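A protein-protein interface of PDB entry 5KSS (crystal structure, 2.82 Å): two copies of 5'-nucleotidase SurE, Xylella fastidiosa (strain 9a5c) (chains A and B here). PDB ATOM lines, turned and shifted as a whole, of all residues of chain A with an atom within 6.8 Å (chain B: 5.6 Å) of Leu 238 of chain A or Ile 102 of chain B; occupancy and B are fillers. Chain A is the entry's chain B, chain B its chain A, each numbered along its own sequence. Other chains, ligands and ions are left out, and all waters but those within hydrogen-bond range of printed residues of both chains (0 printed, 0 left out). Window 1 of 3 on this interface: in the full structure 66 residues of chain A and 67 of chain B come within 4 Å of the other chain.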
ATOM      1  N   SER A  45     -22.535  -3.948 -30.891  1.00  0.00           N
ATOM      2  CA  SER A  45     -22.617  -5.393 -30.696  1.00  0.00           C
ATOM      3  C   SER A  45     -21.318  -6.102 -31.064  1.00  0.00           C
ATOM      4  O   SER A  45     -20.537  -5.609 -31.881  1.00  0.00           O
ATOM      5  CB  SER A  45     -23.771  -5.978 -31.513  1.00  0.00           C
ATOM      6  OG  SER A  45     -25.015  -5.448 -31.092  1.00  0.00           O
ATOM      7  N   ILE A 102     -26.301   4.564 -22.705  1.00  0.00           N
ATOM      8  CA  ILE A 102     -26.676   3.207 -23.083  1.00  0.00           C
ATOM      9  C   ILE A 102     -26.202   2.842 -24.492  1.00  0.00           C
ATOM     10  O   ILE A 102     -25.871   1.689 -24.768  1.00  0.00           O
ATOM     11  CB  ILE A 102     -28.201   2.972 -22.926  1.00  0.00           C
ATOM     12  CG1 ILE A 102     -28.561   1.519 -23.247  1.00  0.00           C
ATOM     13  CG2 ILE A 102     -28.993   3.944 -23.786  1.00  0.00           C
ATOM     14  CD1 ILE A 102     -29.987   1.160 -22.914  1.00  0.00           C
ATOM     15  N   TYR A 103     -26.140   3.835 -25.373  1.00  0.00           N
ATOM     16  CA  TYR A 103     -25.757   3.597 -26.759  1.00  0.00           C
ATOM     17  C   TYR A 103     -24.327   4.053 -27.035  1.00  0.00           C
ATOM     18  O   TYR A 103     -23.852   3.977 -28.168  1.00  0.00           O
ATOM     19  CB  TYR A 103     -26.728   4.306 -27.705  1.00  0.00           C
ATOM     20  CG  TYR A 103     -28.181   4.000 -27.420  1.00  0.00           C
ATOM     21  CD1 TYR A 103     -28.592   2.710 -27.113  1.00  0.00           C
ATOM     22  CD2 TYR A 103     -29.139   5.005 -27.443  1.00  0.00           C
ATOM     23  CE1 TYR A 103     -29.918   2.426 -26.846  1.00  0.00           C
ATOM     24  CE2 TYR A 103     -30.468   4.732 -27.176  1.00  0.00           C
ATOM     25  CZ  TYR A 103     -30.851   3.441 -26.879  1.00  0.00           C
ATOM     26  OH  TYR A 103     -32.171   3.168 -26.612  1.00  0.00           O
ATOM     27  N   MET A 111     -18.314  -1.781 -20.781  1.00  0.00           N
ATOM     28  CA  MET A 111     -19.365  -2.753 -20.519  1.00  0.00           C
ATOM     29  C   MET A 111     -18.863  -4.161 -20.820  1.00  0.00           C
ATOM     30  O   MET A 111     -19.220  -5.121 -20.136  1.00  0.00           O
ATOM     31  CB  MET A 111     -20.601  -2.447 -21.366  1.00  0.00           C
ATOM     32  CG  MET A 111     -21.825  -3.266 -20.996  1.00  0.00           C
ATOM     33  SD  MET A 111     -22.484  -2.817 -19.382  1.00  0.00           S
ATOM     34  CE  MET A 111     -23.004  -1.131 -19.690  1.00  0.00           C
ATOM     35  N   PHE A 115     -18.216  -7.831 -18.249  1.00  0.00           N
ATOM     36  CA  PHE A 115     -18.764  -9.109 -18.700  1.00  0.00           C
ATOM     37  C   PHE A 115     -17.736 -10.235 -18.637  1.00  0.00           C
ATOM     38  O   PHE A 115     -18.094 -11.408 -18.527  1.00  0.00           O
ATOM     39  CB  PHE A 115     -19.323  -8.989 -20.120  1.00  0.00           C
ATOM     40  CG  PHE A 115     -20.593  -8.196 -20.205  1.00  0.00           C
ATOM     41  CD1 PHE A 115     -21.370  -7.986 -19.079  1.00  0.00           C
ATOM     42  CD2 PHE A 115     -21.014  -7.664 -21.412  1.00  0.00           C
ATOM     43  CE1 PHE A 115     -22.540  -7.260 -19.154  1.00  0.00           C
ATOM     44  CE2 PHE A 115     -22.186  -6.935 -21.493  1.00  0.00           C
ATOM     45  CZ  PHE A 115     -22.949  -6.733 -20.361  1.00  0.00           C
ATOM     46  N   HIS A 235     -25.285   0.113 -14.222  1.00  0.00           N
ATOM     47  CA  HIS A 235     -25.513  -1.326 -14.256  1.00  0.00           C
ATOM     48  C   HIS A 235     -24.731  -2.000 -15.374  1.00  0.00           C
ATOM     49  O   HIS A 235     -24.409  -1.381 -16.386  1.00  0.00           O
ATOM     50  CB  HIS A 235     -27.002  -1.632 -14.434  1.00  0.00           C
ATOM     51  CG  HIS A 235     -27.818  -1.422 -13.197  1.00  0.00           C
ATOM     52  ND1 HIS A 235     -27.705  -2.227 -12.085  1.00  0.00           N
ATOM     53  CD2 HIS A 235     -28.773  -0.508 -12.903  1.00  0.00           C
ATOM     54  CE1 HIS A 235     -28.547  -1.813 -11.155  1.00  0.00           C
ATOM     55  NE2 HIS A 235     -29.208  -0.771 -11.628  1.00  0.00           N
ATOM     56  N   VAL A 236     -24.431  -3.278 -15.176  1.00  0.00           N
ATOM     57  CA  VAL A 236     -23.837  -4.100 -16.218  1.00  0.00           C
ATOM     58  C   VAL A 236     -24.857  -5.154 -16.618  1.00  0.00           C
ATOM     59  O   VAL A 236     -24.739  -5.794 -17.661  1.00  0.00           O
ATOM     60  CB  VAL A 236     -22.543  -4.773 -15.733  1.00  0.00           C
ATOM     61  CG1 VAL A 236     -21.579  -3.725 -15.207  1.00  0.00           C
ATOM     62  CG2 VAL A 236     -22.848  -5.801 -14.656  1.00  0.00           C
ATOM     63  N   ASP A 237     -25.866  -5.320 -15.770  1.00  0.00           N
ATOM     64  CA  ASP A 237     -26.967  -6.232 -16.036  1.00  0.00           C
ATOM     65  C   ASP A 237     -28.245  -5.417 -16.179  1.00  0.00           C
ATOM     66  O   ASP A 237     -28.698  -4.787 -15.223  1.00  0.00           O
ATOM     67  CB  ASP A 237     -27.113  -7.239 -14.893  1.00  0.00           C
ATOM     68  CG  ASP A 237     -28.033  -8.395 -15.241  1.00  0.00           C
ATOM     69  OD1 ASP A 237     -28.750  -8.312 -16.262  1.00  0.00           O
ATOM     70  OD2 ASP A 237     -28.042  -9.390 -14.488  1.00  0.00           O
ATOM     71  N   LEU A 238     -28.824  -5.433 -17.374  1.00  0.00           N
ATOM     72  CA  LEU A 238     -30.033  -4.659 -17.636  1.00  0.00           C
ATOM     73  C   LEU A 238     -31.254  -5.226 -16.923  1.00  0.00           C
ATOM     74  O   LEU A 238     -32.256  -4.534 -16.765  1.00  0.00           O
ATOM     75  CB  LEU A 238     -30.304  -4.555 -19.137  1.00  0.00           C
ATOM     76  CG  LEU A 238     -29.378  -3.646 -19.942  1.00  0.00           C
ATOM     77  CD1 LEU A 238     -29.951  -3.416 -21.329  1.00  0.00           C
ATOM     78  CD2 LEU A 238     -29.161  -2.324 -19.225  1.00  0.00           C
ATOM     79  N   THR A 239     -31.164  -6.482 -16.496  1.00  0.00           N
ATOM     80  CA  THR A 239     -32.263  -7.137 -15.792  1.00  0.00           C
ATOM     81  C   THR A 239     -32.666  -6.371 -14.538  1.00  0.00           C
ATOM     82  O   THR A 239     -31.843  -6.133 -13.655  1.00  0.00           O
ATOM     83  CB  THR A 239     -31.898  -8.574 -15.380  1.00  0.00           C
ATOM     84  OG1 THR A 239     -31.549  -9.336 -16.540  1.00  0.00           O
ATOM     85  CG2 THR A 239     -33.068  -9.240 -14.673  1.00  0.00           C
ATOM     86  N   ARG A 240     -33.935  -5.983 -14.469  1.00  0.00           N
ATOM     87  CA  ARG A 240     -34.459  -5.330 -13.279  1.00  0.00           C
ATOM     88  C   ARG A 240     -34.937  -6.383 -12.287  1.00  0.00           C
ATOM     89  O   ARG A 240     -36.093  -6.807 -12.322  1.00  0.00           O
ATOM     90  CB  ARG A 240     -35.595  -4.374 -13.639  1.00  0.00           C
ATOM     91  CG  ARG A 240     -36.072  -3.532 -12.467  1.00  0.00           C
ATOM     92  CD  ARG A 240     -37.027  -2.446 -12.919  1.00  0.00           C
ATOM     93  NE  ARG A 240     -37.389  -1.551 -11.825  1.00  0.00           N
ATOM     94  CZ  ARG A 240     -36.683  -0.481 -11.475  1.00  0.00           C
ATOM     95  NH1 ARG A 240     -35.577  -0.170 -12.135  1.00  0.00           N
ATOM     96  NH2 ARG A 240     -37.083   0.279 -10.465  1.00  0.00           N
ATOM     97  N   TYR A 241     -34.034  -6.802 -11.408  1.00  0.00           N
ATOM     98  CA  TYR A 241     -34.309  -7.883 -10.469  1.00  0.00           C
ATOM     99  C   TYR A 241     -35.391  -7.530  -9.454  1.00  0.00           C
ATOM    100  O   TYR A 241     -36.052  -8.415  -8.910  1.00  0.00           O
ATOM    101  CB  TYR A 241     -33.022  -8.306  -9.755  1.00  0.00           C
ATOM    102  CG  TYR A 241     -32.012  -8.964 -10.667  1.00  0.00           C
ATOM    103  CD1 TYR A 241     -31.093  -8.206 -11.382  1.00  0.00           C
ATOM    104  CD2 TYR A 241     -31.978 -10.344 -10.817  1.00  0.00           C
ATOM    105  CE1 TYR A 241     -30.170  -8.805 -12.218  1.00  0.00           C
ATOM    106  CE2 TYR A 241     -31.060 -10.950 -11.650  1.00  0.00           C
ATOM    107  CZ  TYR A 241     -30.159 -10.178 -12.348  1.00  0.00           C
ATOM    108  OH  TYR A 241     -29.243 -10.784 -13.178  1.00  0.00           O
ATOM    109  N   ASN B  44     -27.794   3.345 -32.146  1.00  0.00           N
ATOM    110  CA  ASN B  44     -29.175   3.482 -31.706  1.00  0.00           C
ATOM    111  C   ASN B  44     -29.460   4.858 -31.116  1.00  0.00           C
ATOM    112  O   ASN B  44     -30.596   5.164 -30.762  1.00  0.00           O
ATOM    113  CB  ASN B  44     -29.523   2.399 -30.684  1.00  0.00           C
ATOM    114  CG  ASN B  44     -29.484   1.005 -31.276  1.00  0.00           C
ATOM    115  OD1 ASN B  44     -29.670   0.824 -32.478  1.00  0.00           O
ATOM    116  ND2 ASN B  44     -29.247   0.009 -30.429  1.00  0.00           N
ATOM    117  N   GLY B  98     -29.674 -11.843 -23.429  1.00  0.00           N
ATOM    118  CA  GLY B  98     -28.454 -11.558 -22.694  1.00  0.00           C
ATOM    119  C   GLY B  98     -27.792 -10.238 -23.042  1.00  0.00           C
ATOM    120  O   GLY B  98     -28.405  -9.176 -22.935  1.00  0.00           O
ATOM    121  N   ASP B  99     -26.530 -10.309 -23.456  1.00  0.00           N
ATOM    122  CA  ASP B  99     -25.745  -9.114 -23.747  1.00  0.00           C
ATOM    123  C   ASP B  99     -26.133  -8.479 -25.079  1.00  0.00           C
ATOM    124  O   ASP B  99     -25.738  -7.350 -25.375  1.00  0.00           O
ATOM    125  CB  ASP B  99     -24.249  -9.439 -23.739  1.00  0.00           C
ATOM    126  CG  ASP B  99     -23.777  -9.978 -22.401  1.00  0.00           C
ATOM    127  OD1 ASP B  99     -24.414  -9.667 -21.373  1.00  0.00           O
ATOM    128  OD2 ASP B  99     -22.766 -10.711 -22.380  1.00  0.00           O
ATOM    129  N   ASP B 100     -26.907  -9.205 -25.879  1.00  0.00           N
ATOM    130  CA  ASP B 100     -27.355  -8.697 -27.169  1.00  0.00           C
ATOM    131  C   ASP B 100     -28.526  -7.732 -27.004  1.00  0.00           C
ATOM    132  O   ASP B 100     -28.994  -7.138 -27.975  1.00  0.00           O
ATOM    133  CB  ASP B 100     -27.755  -9.853 -28.089  1.00  0.00           C
ATOM    134  N   VAL B 101     -28.989  -7.580 -25.767  1.00  0.00           N
ATOM    135  CA  VAL B 101     -30.145  -6.742 -25.467  1.00  0.00           C
ATOM    136  C   VAL B 101     -29.771  -5.264 -25.354  1.00  0.00           C
ATOM    137  O   VAL B 101     -30.492  -4.394 -25.845  1.00  0.00           O
ATOM    138  CB  VAL B 101     -30.834  -7.199 -24.165  1.00  0.00           C
ATOM    139  CG1 VAL B 101     -32.022  -6.308 -23.841  1.00  0.00           C
ATOM    140  CG2 VAL B 101     -31.270  -8.645 -24.286  1.00  0.00           C
ATOM    141  N   ILE B 102     -28.637  -4.991 -24.712  1.00  0.00           N
ATOM    142  CA  ILE B 102     -28.189  -3.621 -24.475  1.00  0.00           C
ATOM    143  C   ILE B 102     -27.971  -2.852 -25.774  1.00  0.00           C
ATOM    144  O   ILE B 102     -28.204  -1.646 -25.842  1.00  0.00           O
ATOM    145  CB  ILE B 102     -26.864  -3.586 -23.683  1.00  0.00           C
ATOM    146  CG1 ILE B 102     -26.795  -4.734 -22.675  1.00  0.00           C
ATOM    147  CG2 ILE B 102     -26.690  -2.241 -22.992  1.00  0.00           C
ATOM    148  CD1 ILE B 102     -25.511  -4.754 -21.869  1.00  0.00           C
ATOM    149  N   TYR B 103     -27.518  -3.559 -26.804  1.00  0.00           N
ATOM    150  CA  TYR B 103     -27.173  -2.927 -28.071  1.00  0.00           C
ATOM    151  C   TYR B 103     -28.243  -3.175 -29.129  1.00  0.00           C
ATOM    152  O   TYR B 103     -28.103  -2.754 -30.277  1.00  0.00           O
ATOM    153  CB  TYR B 103     -25.816  -3.438 -28.562  1.00  0.00           C
ATOM    154  CG  TYR B 103     -24.720  -3.336 -27.526  1.00  0.00           C
ATOM    155  CD1 TYR B 103     -24.602  -2.211 -26.718  1.00  0.00           C
ATOM    156  CD2 TYR B 103     -23.810  -4.369 -27.345  1.00  0.00           C
ATOM    157  CE1 TYR B 103     -23.604  -2.114 -25.765  1.00  0.00           C
ATOM    158  CE2 TYR B 103     -22.807  -4.283 -26.396  1.00  0.00           C
ATOM    159  CZ  TYR B 103     -22.710  -3.153 -25.610  1.00  0.00           C
ATOM    160  OH  TYR B 103     -21.715  -3.065 -24.662  1.00  0.00           O
ATOM    161  N   SER B 104     -29.313  -3.860 -28.733  1.00  0.00           N
ATOM    162  CA  SER B 104     -30.408  -4.173 -29.645  1.00  0.00           C
ATOM    163  C   SER B 104     -31.162  -2.921 -30.082  1.00  0.00           C
ATOM    164  O   SER B 104     -31.554  -2.097 -29.254  1.00  0.00           O
ATOM    165  CB  SER B 104     -31.378  -5.163 -28.993  1.00  0.00           C
ATOM    166  OG  SER B 104     -32.532  -5.348 -29.795  1.00  0.00           O
ATOM    167  N   MET B 111     -36.940   1.215 -25.335  1.00  0.00           N
ATOM    168  CA  MET B 111     -36.225   1.995 -24.335  1.00  0.00           C
ATOM    169  C   MET B 111     -36.607   3.466 -24.447  1.00  0.00           C
ATOM    170  O   MET B 111     -36.698   4.177 -23.445  1.00  0.00           O
ATOM    171  CB  MET B 111     -34.716   1.827 -24.509  1.00  0.00           C
ATOM    172  CG  MET B 111     -33.893   2.415 -23.374  1.00  0.00           C
ATOM    173  SD  MET B 111     -34.097   1.496 -21.837  1.00  0.00           S
ATOM    174  CE  MET B 111     -33.391  -0.083 -22.297  1.00  0.00           C
ATOM    175  N   LEU B 183     -31.704 -11.774 -17.888  1.00  0.00           N
ATOM    176  CA  LEU B 183     -30.769 -11.778 -19.006  1.00  0.00           C
ATOM    177  C   LEU B 183     -29.598 -12.707 -18.720  1.00  0.00           C
ATOM    178  O   LEU B 183     -29.167 -12.842 -17.575  1.00  0.00           O
ATOM    179  CB  LEU B 183     -30.261 -10.366 -19.296  1.00  0.00           C
ATOM    180  CG  LEU B 183     -31.308  -9.355 -19.763  1.00  0.00           C
ATOM    181  CD1 LEU B 183     -30.664  -8.014 -20.048  1.00  0.00           C
ATOM    182  CD2 LEU B 183     -32.040  -9.870 -20.990  1.00  0.00           C
ATOM    183  N   PRO B 233     -38.023  -8.459 -17.703  1.00  0.00           N
ATOM    184  CA  PRO B 233     -38.168  -7.060 -17.288  1.00  0.00           C
ATOM    185  C   PRO B 233     -36.794  -6.424 -17.107  1.00  0.00           C
ATOM    186  O   PRO B 233     -36.047  -6.804 -16.205  1.00  0.00           O
ATOM    187  CB  PRO B 233     -38.896  -7.165 -15.944  1.00  0.00           C
ATOM    188  CG  PRO B 233     -38.574  -8.530 -15.441  1.00  0.00           C
ATOM    189  CD  PRO B 233     -38.447  -9.402 -16.655  1.00  0.00           C
ATOM    190  N   ILE B 234     -36.459  -5.472 -17.971  1.00  0.00           N
ATOM    191  CA  ILE B 234     -35.136  -4.861 -17.936  1.00  0.00           C
ATOM    192  C   ILE B 234     -35.170  -3.408 -17.477  1.00  0.00           C
ATOM    193  O   ILE B 234     -36.205  -2.744 -17.550  1.00  0.00           O
ATOM    194  CB  ILE B 234     -34.428  -4.952 -19.303  1.00  0.00           C
ATOM    195  CG1 ILE B 234     -35.183  -4.139 -20.351  1.00  0.00           C
ATOM    196  CG2 ILE B 234     -34.301  -6.405 -19.740  1.00  0.00           C
ATOM    197  CD1 ILE B 234     -34.518  -4.125 -21.707  1.00  0.00           C
ATOM    198  N   HIS B 235     -34.028  -2.925 -16.998  1.00  0.00           N
ATOM    199  CA  HIS B 235     -33.912  -1.554 -16.517  1.00  0.00           C
ATOM    200  C   HIS B 235     -34.080  -0.546 -17.644  1.00  0.00           C
ATOM    201  O   HIS B 235     -33.815  -0.846 -18.808  1.00  0.00           O
ATOM    202  CB  HIS B 235     -32.554  -1.330 -15.846  1.00  0.00           C
ATOM    203  CG  HIS B 235     -32.445  -1.929 -14.480  1.00  0.00           C
ATOM    204  ND1 HIS B 235     -33.149  -1.448 -13.397  1.00  0.00           N
ATOM    205  CD2 HIS B 235     -31.701  -2.961 -14.015  1.00  0.00           C
ATOM    206  CE1 HIS B 235     -32.850  -2.162 -12.328  1.00  0.00           C
ATOM    207  NE2 HIS B 235     -31.974  -3.087 -12.675  1.00  0.00           N
ATOM    208  N   LEU B 238     -29.778   2.967 -16.332  1.00  0.00           N
ATOM    209  CA  LEU B 238     -28.552   2.193 -16.174  1.00  0.00           C
ATOM    210  C   LEU B 238     -27.878   2.451 -14.829  1.00  0.00           C
ATOM    211  O   LEU B 238     -27.043   1.663 -14.394  1.00  0.00           O
ATOM    212  CB  LEU B 238     -27.581   2.463 -17.328  1.00  0.00           C
ATOM    213  CG  LEU B 238     -27.760   1.623 -18.599  1.00  0.00           C
ATOM    214  CD1 LEU B 238     -29.117   1.856 -19.252  1.00  0.00           C
ATOM    215  CD2 LEU B 238     -26.637   1.899 -19.588  1.00  0.00           C
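Among the printed residues, pairs that only touch across the chains: Leu 238 of chain A with Ile 234 of chain B, Ser 45 of chain A with Tyr 103 of chain B, Phe 115 of chain A with Asp 99 of chain B, Met 111 of chain A with Tyr 103 of chain B, Tyr 103 of chain A with Met 111 of chain B, Phe 115 of chain A with Ile 102 of chain B, Leu 238 of chain A with Leu 183 of chain B, Leu 238 of chain A with Ile 102 of chain B, Tyr 103 of chain A with Asn 44 of chain B, Ile 102 of chain A with Met 111 of chain B, Asp 237 of chain A with His 235 of chain B, Ile 102 of chain A with Leu 238 of chain B, His 235 of chain A with His 235 of chain B, Thr 239 of chain A with Pro 233 of chain B, Arg 240 of chain A with Ile 234 of chain B and Asp 237 of chain A with Leu 183 of chain B.
Of chain B, only Ile 102, Leu 183, Ile 234 and His 235 come within 4 Å of Leu 238 of chain A.
Of chain A, only Phe 115 (3.6 Å) and Leu 238 (3.6 Å) come within 4 Å of Ile 102 of chain B.
Of the printed residues of chain A, Leu 183 of chain B touches Asp 237, Leu 238 and Thr 239.
Printed residues of chain B within 4 Å of Met 111 of chain A: Tyr 103.
Of the printed residues of chain A, Ile 234 of chain B touches Leu 238 and Arg 240.
Printed residues of chain A within 4 Å of Asp 99 of chain B: Phe 115.
The nearest residue of chain A that does not touch Ile 102 of chain B is Met 111 of chain A (4.1 Å).
The nearest printed residue of chain B that does not touch Phe 115 of chain A is Tyr 103 of chain B (5.0 Å).
Of the 12 printed residues of chain A, 10 touch a printed residue of chain B.
Hydrophobic or aromatic side chains of chain A within 4 Å of the printed part of chain B: Ile 102, Tyr 103, Met 111, Phe 115, His 235 and Leu 238.
Printed residues of chain B that touch a printed residue of chain A: Asn 44, Asp 99, Ile 102, Tyr 103, Met 111, Leu 183, Pro 233, Ile 234, His 235 and Leu 238.
Hydrophobic or aromatic side chains of chain B within 4 Å of the printed part of chain A: Ile 102, Tyr 103, Met 111, Leu 183, Ile 234, His 235 and Leu 238.
Along chain B the printed residues that touch a printed residue of chain A span positions 44 to 238.
Among the printed residues, no Asp or Glu carboxylate lies within 4 Å of a Lys or Arg side-chain nitrogen of the other chain.
ND2 of Asn 44 of chain B lies within hydrogen-bond range of O of Tyr 103 of chain B (3.0 Å).
ND2 of Asn 44 of chain B lies within hydrogen-bond range of O of Ser 104 of chain B, 3.3 Å away.
The side-chain carboxylate of Asp 237 of chain A lies within hydrogen-bond range of the side-chain hydroxyl of Thr 239 of chain A, at 3.0 Å.
Ile 102 of chain A touches Met 111 of chain B, but with the chains exchanged Met 111 of chain A does not touch Ile 102 of chain B (4.1 Å).
Tyr 103 of chain A touches Met 111 of chain B, and with the chains exchanged Met 111 of chain A touches Tyr 103 of chain B.
His 235 of chain A touches its own counterpart, His 235 of chain B.
His 235 of chain A touches Leu 238 of chain B, and with the chains exchanged Leu 238 of chain A touches His 235 of chain B.
Of the 22 pairs that touch across the chains among the printed residues, 7 have their exchanged pair printed and touching as well.
The backbone NH (N) of Leu 183 of chain B sits at hydrogen-bond distance from the side-chain hydroxyl (OG1) of Thr 239 of chain A.
The backbone NH of Arg 240 of chain A is in hydrogen-bond range of the backbone carbonyl oxygen of Pro 233 of chain B (2.9 Å).
The backbone carbonyl oxygen (O) of Leu 238 of chain A is in hydrogen-bond range of the backbone NH (N) of His 235 of chain B (2.4 Å).
The backbone carbonyl oxygen (O) of Thr 239 of chain A sits close to a ring nitrogen (NE2) of His 235 of chain B (3.2 Å).
ND1 of His 235 of chain B sits at hydrogen-bond distance from NH1 of Arg 240 of chain A (3.0 Å).
The backbone NH (N) of His 235 of chain A sits close to the backbone carbonyl oxygen (O) of Leu 238 of chain B (2.4 Å).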
